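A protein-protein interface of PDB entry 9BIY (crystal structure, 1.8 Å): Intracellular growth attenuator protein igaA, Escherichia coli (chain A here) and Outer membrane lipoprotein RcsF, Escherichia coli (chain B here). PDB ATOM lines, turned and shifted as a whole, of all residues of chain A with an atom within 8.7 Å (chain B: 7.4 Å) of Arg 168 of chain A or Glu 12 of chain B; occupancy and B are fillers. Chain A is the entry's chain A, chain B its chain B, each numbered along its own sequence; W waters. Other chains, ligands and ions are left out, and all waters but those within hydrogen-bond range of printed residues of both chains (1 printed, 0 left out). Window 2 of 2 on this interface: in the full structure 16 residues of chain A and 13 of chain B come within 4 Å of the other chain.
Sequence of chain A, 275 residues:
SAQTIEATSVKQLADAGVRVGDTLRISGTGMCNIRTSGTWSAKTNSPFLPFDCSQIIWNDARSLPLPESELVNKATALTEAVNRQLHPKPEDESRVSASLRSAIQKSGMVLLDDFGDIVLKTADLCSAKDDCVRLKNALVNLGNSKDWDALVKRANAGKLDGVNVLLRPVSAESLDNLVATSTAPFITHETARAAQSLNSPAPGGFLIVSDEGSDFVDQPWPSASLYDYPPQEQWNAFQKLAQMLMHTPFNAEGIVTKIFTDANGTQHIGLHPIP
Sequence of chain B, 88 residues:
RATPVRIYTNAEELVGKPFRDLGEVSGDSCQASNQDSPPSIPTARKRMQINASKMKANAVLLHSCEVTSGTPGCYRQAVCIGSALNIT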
ATOM      1  N   LEU A  86      17.865  14.279 -32.899  1.00  0.00           N
ATOM      2  CA  LEU A  86      16.726  15.112 -33.274  1.00  0.00           C
ATOM      3  C   LEU A  86      15.824  14.492 -34.339  1.00  0.00           C
ATOM      4  O   LEU A  86      14.664  14.902 -34.451  1.00  0.00           O
ATOM      5  CB  LEU A  86      17.214  16.481 -33.772  1.00  0.00           C
ATOM      6  CG  LEU A  86      18.143  17.236 -32.823  1.00  0.00           C
ATOM      7  CD1 LEU A  86      18.602  18.541 -33.436  1.00  0.00           C
ATOM      8  CD2 LEU A  86      17.446  17.468 -31.475  1.00  0.00           C
ATOM      9  N   ILE A 104       8.911  10.877 -23.001  1.00  0.00           N
ATOM     10  CA  ILE A 104       9.242  12.134 -23.669  1.00  0.00           C
ATOM     11  C   ILE A 104       8.431  12.323 -24.949  1.00  0.00           C
ATOM     12  O   ILE A 104       8.100  13.457 -25.318  1.00  0.00           O
ATOM     13  CB  ILE A 104      10.754  12.196 -23.950  1.00  0.00           C
ATOM     14  CG1 ILE A 104      11.541  12.223 -22.639  1.00  0.00           C
ATOM     15  CG2 ILE A 104      11.101  13.407 -24.800  1.00  0.00           C
ATOM     16  CD1 ILE A 104      11.885  13.597 -22.150  1.00  0.00           C
ATOM     17  N   SER A 107       5.181  13.306 -23.919  1.00  0.00           N
ATOM     18  CA  SER A 107       5.404  14.650 -23.392  1.00  0.00           C
ATOM     19  C   SER A 107       5.174  15.692 -24.475  1.00  0.00           C
ATOM     20  O   SER A 107       4.303  16.560 -24.353  1.00  0.00           O
ATOM     21  CB  SER A 107       6.827  14.794 -22.834  1.00  0.00           C
ATOM     22  OG  SER A 107       7.147  13.785 -21.896  1.00  0.00           O
ATOM     23  N   GLY A 108       5.932  15.594 -25.563  1.00  0.00           N
ATOM     24  CA  GLY A 108       5.943  16.636 -26.564  1.00  0.00           C
ATOM     25  C   GLY A 108       7.066  17.604 -26.272  1.00  0.00           C
ATOM     26  O   GLY A 108       6.824  18.773 -25.956  1.00  0.00           O
ATOM     27  N   MET A 109       8.297  17.092 -26.314  1.00  0.00           N
ATOM     28  CA  MET A 109       9.517  17.869 -26.072  1.00  0.00           C
ATOM     29  C   MET A 109      10.696  17.187 -26.737  1.00  0.00           C
ATOM     30  O   MET A 109      10.521  16.091 -27.310  1.00  0.00           O
ATOM     31  CB  MET A 109       9.766  18.155 -24.592  1.00  0.00           C
ATOM     32  CG  MET A 109       9.427  19.612 -24.270  1.00  0.00           C
ATOM     33  SD  MET A 109      10.562  20.283 -22.813  1.00  0.00           S
ATOM     34  CE  MET A 109      10.382  22.213 -23.136  1.00  0.00           C
ATOM     35  N   VAL A 110      11.890  17.774 -26.653  1.00  0.00           N
ATOM     36  CA  VAL A 110      13.057  17.235 -27.348  1.00  0.00           C
ATOM     37  C   VAL A 110      14.164  16.939 -26.345  1.00  0.00           C
ATOM     38  O   VAL A 110      14.557  17.811 -25.561  1.00  0.00           O
ATOM     39  CB  VAL A 110      13.558  18.185 -28.451  1.00  0.00           C
ATOM     40  CG1 VAL A 110      14.812  17.625 -29.082  1.00  0.00           C
ATOM     41  CG2 VAL A 110      12.488  18.369 -29.517  1.00  0.00           C
ATOM     42  N   LEU A 111      14.682  15.716 -26.407  1.00  0.00           N
ATOM     43  CA  LEU A 111      15.764  15.235 -25.563  1.00  0.00           C
ATOM     44  C   LEU A 111      17.025  15.018 -26.388  1.00  0.00           C
ATOM     45  O   LEU A 111      16.962  14.512 -27.513  1.00  0.00           O
ATOM     46  CB  LEU A 111      15.371  13.915 -24.888  1.00  0.00           C
ATOM     47  CG  LEU A 111      16.466  13.125 -24.169  1.00  0.00           C
ATOM     48  CD1 LEU A 111      16.491  13.490 -22.703  1.00  0.00           C
ATOM     49  CD2 LEU A 111      16.248  11.633 -24.349  1.00  0.00           C
ATOM     50  N   LEU A 142      24.202  24.892 -22.829  1.00  0.00           N
ATOM     51  CA  LEU A 142      23.465  23.696 -22.425  1.00  0.00           C
ATOM     52  C   LEU A 142      24.163  22.959 -21.296  1.00  0.00           C
ATOM     53  O   LEU A 142      23.499  22.362 -20.443  1.00  0.00           O
ATOM     54  CB  LEU A 142      23.299  22.768 -23.623  1.00  0.00           C
ATOM     55  CG  LEU A 142      22.292  23.240 -24.664  1.00  0.00           C
ATOM     56  CD1 LEU A 142      22.379  22.398 -25.920  1.00  0.00           C
ATOM     57  CD2 LEU A 142      20.895  23.193 -24.050  1.00  0.00           C
ATOM     58  N   VAL A 165      20.438  16.001 -22.025  1.00  0.00           N
ATOM     59  CA  VAL A 165      20.032  17.392 -21.880  1.00  0.00           C
ATOM     60  C   VAL A 165      18.664  17.548 -22.525  1.00  0.00           C
ATOM     61  O   VAL A 165      18.434  17.070 -23.640  1.00  0.00           O
ATOM     62  CB  VAL A 165      21.050  18.373 -22.500  1.00  0.00           C
ATOM     63  CG1 VAL A 165      20.630  19.799 -22.229  1.00  0.00           C
ATOM     64  CG2 VAL A 165      22.434  18.141 -21.922  1.00  0.00           C
ATOM     65  N   LEU A 166      17.764  18.201 -21.818  1.00  0.00           N
ATOM     66  CA  LEU A 166      16.420  18.495 -22.288  1.00  0.00           C
ATOM     67  C   LEU A 166      16.389  19.956 -22.704  1.00  0.00           C
ATOM     68  O   LEU A 166      16.884  20.820 -21.975  1.00  0.00           O
ATOM     69  CB  LEU A 166      15.403  18.242 -21.175  1.00  0.00           C
ATOM     70  CG  LEU A 166      14.034  17.618 -21.415  1.00  0.00           C
ATOM     71  CD1 LEU A 166      14.160  16.326 -22.184  1.00  0.00           C
ATOM     72  CD2 LEU A 166      13.427  17.355 -20.059  1.00  0.00           C
ATOM     73  N   LEU A 167      15.834  20.229 -23.873  1.00  0.00           N
ATOM     74  CA  LEU A 167      15.743  21.598 -24.343  1.00  0.00           C
ATOM     75  C   LEU A 167      14.429  21.762 -25.092  1.00  0.00           C
ATOM     76  O   LEU A 167      13.820  20.783 -25.540  1.00  0.00           O
ATOM     77  CB  LEU A 167      16.959  21.990 -25.199  1.00  0.00           C
ATOM     78  CG  LEU A 167      17.213  21.309 -26.537  1.00  0.00           C
ATOM     79  CD1 LEU A 167      18.380  21.976 -27.282  1.00  0.00           C
ATOM     80  CD2 LEU A 167      17.500  19.837 -26.362  1.00  0.00           C
ATOM     81  N   ARG A 168      13.958  23.012 -25.167  1.00  0.00           N
ATOM     82  CA  ARG A 168      12.674  23.127 -25.835  1.00  0.00           C
ATOM     83  C   ARG A 168      12.856  23.273 -27.343  1.00  0.00           C
ATOM     84  O   ARG A 168      13.894  23.761 -27.806  1.00  0.00           O
ATOM     85  CB  ARG A 168      11.880  24.303 -25.299  1.00  0.00           C
ATOM     86  CG  ARG A 168      12.513  25.638 -25.487  1.00  0.00           C
ATOM     87  CD  ARG A 168      12.424  26.420 -24.193  1.00  0.00           C
ATOM     88  NE  ARG A 168      11.184  26.146 -23.476  1.00  0.00           N
ATOM     89  CZ  ARG A 168      11.021  26.415 -22.186  1.00  0.00           C
ATOM     90  NH1 ARG A 168      12.023  26.957 -21.510  1.00  0.00           N
ATOM     91  NH2 ARG A 168       9.876  26.151 -21.574  1.00  0.00           N
ATOM     92  N   PRO A 169      11.839  22.866 -28.120  1.00  0.00           N
ATOM     93  CA  PRO A 169      12.004  22.801 -29.583  1.00  0.00           C
ATOM     94  C   PRO A 169      12.636  24.033 -30.216  1.00  0.00           C
ATOM     95  O   PRO A 169      13.389  23.884 -31.183  1.00  0.00           O
ATOM     96  CB  PRO A 169      10.567  22.583 -30.066  1.00  0.00           C
ATOM     97  CG  PRO A 169       9.941  21.796 -28.985  1.00  0.00           C
ATOM     98  CD  PRO A 169      10.507  22.380 -27.709  1.00  0.00           C
ATOM     99  N   VAL A 170      12.371  25.236 -29.705  1.00  0.00           N
ATOM    100  CA  VAL A 170      12.980  26.418 -30.312  1.00  0.00           C
ATOM    101  C   VAL A 170      14.497  26.361 -30.182  1.00  0.00           C
ATOM    102  O   VAL A 170      15.226  26.726 -31.112  1.00  0.00           O
ATOM    103  CB  VAL A 170      12.410  27.713 -29.706  1.00  0.00           C
ATOM    104  CG1 VAL A 170      11.013  27.983 -30.250  1.00  0.00           C
ATOM    105  CG2 VAL A 170      12.411  27.653 -28.190  1.00  0.00           C
ATOM    106  N   SER A 171      14.998  25.893 -29.035  1.00  0.00           N
ATOM    107  CA  SER A 171      16.443  25.744 -28.890  1.00  0.00           C
ATOM    108  C   SER A 171      16.966  24.568 -29.699  1.00  0.00           C
ATOM    109  O   SER A 171      18.102  24.615 -30.183  1.00  0.00           O
ATOM    110  CB  SER A 171      16.825  25.578 -27.423  1.00  0.00           C
ATOM    111  OG  SER A 171      16.240  26.588 -26.623  1.00  0.00           O
ATOM    112  N   ALA A 172      16.157  23.514 -29.848  1.00  0.00           N
ATOM    113  CA  ALA A 172      16.570  22.343 -30.614  1.00  0.00           C
ATOM    114  C   ALA A 172      16.664  22.664 -32.095  1.00  0.00           C
ATOM    115  O   ALA A 172      17.521  22.118 -32.801  1.00  0.00           O
ATOM    116  CB  ALA A 172      15.591  21.195 -30.384  1.00  0.00           C
ATOM    117  N   GLU A 173      15.784  23.537 -32.589  1.00  0.00           N
ATOM    118  CA  GLU A 173      15.862  23.934 -33.988  1.00  0.00           C
ATOM    119  C   GLU A 173      16.976  24.946 -34.211  1.00  0.00           C
ATOM    120  O   GLU A 173      17.674  24.887 -35.228  1.00  0.00           O
ATOM    121  CB  GLU A 173      14.516  24.483 -34.459  1.00  0.00           C
ATOM    122  CG  GLU A 173      13.672  23.454 -35.207  1.00  0.00           C
ATOM    123  CD  GLU A 173      14.063  23.310 -36.674  1.00  0.00           C
ATOM    124  OE1 GLU A 173      13.175  22.985 -37.493  1.00  0.00           O
ATOM    125  OE2 GLU A 173      15.253  23.516 -37.013  1.00  0.00           O
ATOM    126  N   SER A 174      17.167  25.875 -33.270  1.00  0.00           N
ATOM    127  CA  SER A 174      18.362  26.708 -33.315  1.00  0.00           C
ATOM    128  C   SER A 174      19.626  25.849 -33.312  1.00  0.00           C
ATOM    129  O   SER A 174      20.590  26.145 -34.022  1.00  0.00           O
ATOM    130  CB  SER A 174      18.361  27.693 -32.143  1.00  0.00           C
ATOM    131  OG  SER A 174      19.450  28.597 -32.230  1.00  0.00           O
ATOM    132  N   LEU A 175      19.627  24.757 -32.541  1.00  0.00           N
ATOM    133  CA  LEU A 175      20.807  23.901 -32.485  1.00  0.00           C
ATOM    134  C   LEU A 175      20.993  23.135 -33.790  1.00  0.00           C
ATOM    135  O   LEU A 175      22.090  23.119 -34.360  1.00  0.00           O
ATOM    136  CB  LEU A 175      20.705  22.938 -31.302  1.00  0.00           C
ATOM    137  CG  LEU A 175      21.815  21.887 -31.200  1.00  0.00           C
ATOM    138  CD1 LEU A 175      23.157  22.565 -30.947  1.00  0.00           C
ATOM    139  CD2 LEU A 175      21.494  20.885 -30.095  1.00  0.00           C
ATOM    140  N   TYR B   8       9.954  16.431  -9.994  1.00  0.00           N
ATOM    141  CA  TYR B   8       9.509  17.291 -11.081  1.00  0.00           C
ATOM    142  C   TYR B   8       8.264  16.693 -11.723  1.00  0.00           C
ATOM    143  O   TYR B   8       8.180  15.477 -11.925  1.00  0.00           O
ATOM    144  CB  TYR B   8      10.610  17.464 -12.140  1.00  0.00           C
ATOM    145  CG  TYR B   8      11.867  18.141 -11.631  1.00  0.00           C
ATOM    146  CD1 TYR B   8      12.938  17.397 -11.155  1.00  0.00           C
ATOM    147  CD2 TYR B   8      11.983  19.525 -11.634  1.00  0.00           C
ATOM    148  CE1 TYR B   8      14.088  18.014 -10.692  1.00  0.00           C
ATOM    149  CE2 TYR B   8      13.128  20.150 -11.174  1.00  0.00           C
ATOM    150  CZ  TYR B   8      14.177  19.393 -10.703  1.00  0.00           C
ATOM    151  OH  TYR B   8      15.317  20.022 -10.244  1.00  0.00           O
ATOM    152  N   THR B   9       7.301  17.555 -12.053  1.00  0.00           N
ATOM    153  CA  THR B   9       6.041  17.119 -12.639  1.00  0.00           C
ATOM    154  C   THR B   9       5.955  17.381 -14.133  1.00  0.00           C
ATOM    155  O   THR B   9       5.116  16.772 -14.805  1.00  0.00           O
ATOM    156  CB  THR B   9       4.859  17.804 -11.934  1.00  0.00           C
ATOM    157  OG1 THR B   9       5.024  19.231 -11.982  1.00  0.00           O
ATOM    158  CG2 THR B   9       4.798  17.370 -10.497  1.00  0.00           C
ATOM    159  N   ASN B  10       6.804  18.263 -14.662  1.00  0.00           N
ATOM    160  CA  ASN B  10       6.870  18.560 -16.082  1.00  0.00           C
ATOM    161  C   ASN B  10       8.314  18.470 -16.541  1.00  0.00           C
ATOM    162  O   ASN B  10       9.224  18.943 -15.850  1.00  0.00           O
ATOM    163  CB  ASN B  10       6.336  19.957 -16.399  1.00  0.00           C
ATOM    164  CG  ASN B  10       4.887  19.945 -16.813  1.00  0.00           C
ATOM    165  OD1 ASN B  10       4.078  19.186 -16.275  1.00  0.00           O
ATOM    166  ND2 ASN B  10       4.544  20.796 -17.772  1.00  0.00           N
ATOM    167  N   ALA B  11       8.515  17.868 -17.716  1.00  0.00           N
ATOM    168  CA  ALA B  11       9.836  17.864 -18.328  1.00  0.00           C
ATOM    169  C   ALA B  11      10.376  19.278 -18.477  1.00  0.00           C
ATOM    170  O   ALA B  11      11.583  19.502 -18.328  1.00  0.00           O
ATOM    171  CB  ALA B  11       9.780  17.168 -19.686  1.00  0.00           C
ATOM    172  N   GLU B  12       9.499  20.237 -18.730  1.00  0.00           N
ATOM    173  CA  GLU B  12       9.928  21.619 -18.897  1.00  0.00           C
ATOM    174  C   GLU B  12      10.744  22.154 -17.718  1.00  0.00           C
ATOM    175  O   GLU B  12      11.497  23.114 -17.867  1.00  0.00           O
ATOM    176  CB  GLU B  12       8.727  22.525 -19.164  1.00  0.00           C
ATOM    177  CG  GLU B  12       7.859  22.080 -20.329  1.00  0.00           C
ATOM    178  CD  GLU B  12       7.670  23.172 -21.362  1.00  0.00           C
ATOM    179  OE1 GLU B  12       8.319  24.230 -21.232  1.00  0.00           O
ATOM    180  OE2 GLU B  12       6.873  22.976 -22.303  1.00  0.00           O
ATOM    181  N   GLU B  13      10.609  21.534 -16.552  1.00  0.00           N
ATOM    182  CA  GLU B  13      11.331  22.001 -15.380  1.00  0.00           C
ATOM    183  C   GLU B  13      12.791  21.560 -15.358  1.00  0.00           C
ATOM    184  O   GLU B  13      13.574  22.110 -14.577  1.00  0.00           O
ATOM    185  CB  GLU B  13      10.592  21.533 -14.122  1.00  0.00           C
ATOM    186  CG  GLU B  13       9.139  21.994 -14.104  1.00  0.00           C
ATOM    187  CD  GLU B  13       8.261  21.205 -13.123  1.00  0.00           C
ATOM    188  OE1 GLU B  13       8.744  20.208 -12.540  1.00  0.00           O
ATOM    189  OE2 GLU B  13       7.082  21.587 -12.934  1.00  0.00           O
ATOM    190  N   LEU B  14      13.182  20.611 -16.206  1.00  0.00           N
ATOM    191  CA  LEU B  14      14.561  20.150 -16.289  1.00  0.00           C
ATOM    192  C   LEU B  14      15.324  20.750 -17.463  1.00  0.00           C
ATOM    193  O   LEU B  14      16.512  20.456 -17.621  1.00  0.00           O
ATOM    194  CB  LEU B  14      14.596  18.625 -16.392  1.00  0.00           C
ATOM    195  CG  LEU B  14      14.237  17.885 -15.104  1.00  0.00           C
ATOM    196  CD1 LEU B  14      13.611  16.561 -15.467  1.00  0.00           C
ATOM    197  CD2 LEU B  14      15.453  17.692 -14.208  1.00  0.00           C
ATOM    198  N   VAL B  15      14.673  21.571 -18.290  1.00  0.00           N
ATOM    199  CA  VAL B  15      15.350  22.193 -19.422  1.00  0.00           C
ATOM    200  C   VAL B  15      16.574  22.958 -18.938  1.00  0.00           C
ATOM    201  O   VAL B  15      16.491  23.792 -18.029  1.00  0.00           O
ATOM    202  CB  VAL B  15      14.376  23.100 -20.188  1.00  0.00           C
ATOM    203  CG1 VAL B  15      15.119  24.234 -20.873  1.00  0.00           C
ATOM    204  CG2 VAL B  15      13.596  22.284 -21.216  1.00  0.00           C
ATOM    205  N   GLY B  16      17.726  22.664 -19.541  1.00  0.00           N
ATOM    206  CA  GLY B  16      18.960  23.288 -19.114  1.00  0.00           C
ATOM    207  C   GLY B  16      19.517  22.724 -17.832  1.00  0.00           C
ATOM    208  O   GLY B  16      20.110  23.463 -17.037  1.00  0.00           O
ATOM    209  N   LEU B  61      11.393  12.592 -12.446  1.00  0.00           N
ATOM    210  CA  LEU B  61      10.425  13.141 -13.382  1.00  0.00           C
ATOM    211  C   LEU B  61       9.191  12.250 -13.337  1.00  0.00           C
ATOM    212  O   LEU B  61       9.260  11.075 -13.704  1.00  0.00           O
ATOM    213  CB  LEU B  61      11.001  13.203 -14.800  1.00  0.00           C
ATOM    214  CG  LEU B  61       9.988  13.571 -15.886  1.00  0.00           C
ATOM    215  CD1 LEU B  61       9.381  14.944 -15.611  1.00  0.00           C
ATOM    216  CD2 LEU B  61      10.614  13.511 -17.284  1.00  0.00           C
HETATM  217  O   HOH W   1      17.973  18.585 -18.937  1.00  0.00           O
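Water W1 lies within hydrogen-bond range of the backbone carbonyl oxygen (O) of Leu 14 of chain B and the backbone NH (N) of Leu 166 of chain A.
N of Leu 167 of chain A sits at hydrogen-bond distance from O of Val 110 of chain A (3.2 Å).
Of the 19 printed residues of chain A, 4 touch a printed residue of chain B. Printed residues of chain A that touch a printed residue of chain B: Met 109, Leu 166, Leu 167 and Arg 168. Of the 10 printed residues of chain B, 4 touch a printed residue of chain A. Printed residues of chain B that touch a printed residue of chain A: Ala 11, Glu 12, Val 15 and Gly 16. Hydrophobic or aromatic side chains of chain B within 4 Å of the printed part of chain A: Ala 11 and Val 15. Along chain B the printed residues that touch a printed residue of chain A span positions 11 to 16.
Leu 86 of chain A touches none of the printed residues of chain B. Printed residues of chain B within 4 Å of Arg 168 of chain A: Glu 12 (2.5 Å). Pro 169 of chain A touches none of the printed residues of chain B. Of the printed residues of chain A, Ala 11 of chain B touches Leu 166 (3.3 Å). Of the printed residues of chain A, Val 15 of chain B touches Met 109 (3.7 Å), Leu 166 (3.3 Å) and Leu 167 (3.9 Å). Printed residues of chain A within 4 Å of Gly 16 of chain B: Leu 166 (3.2 Å).
Among the printed residues, merely in contact across the chains: Leu 166 of chain A with Val 15 of chain B (3.3 Å), Leu 166 of chain A with Ala 11 of chain B (3.3 Å), Met 109 of chain A with Glu 12 of chain B (3.4 Å), Met 109 of chain A with Val 15 of chain B (3.7 Å) and Leu 167 of chain A with Val 15 of chain B (3.9 Å).
NH2 of Arg 168 of chain A is in salt-bridge range of OE1 of Glu 12 of chain B (2.5 Å). The backbone carbonyl oxygen of Leu 166 of chain A sits at hydrogen-bond distance from the backbone NH of Gly 16 of chain B, at 3.2 Å.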
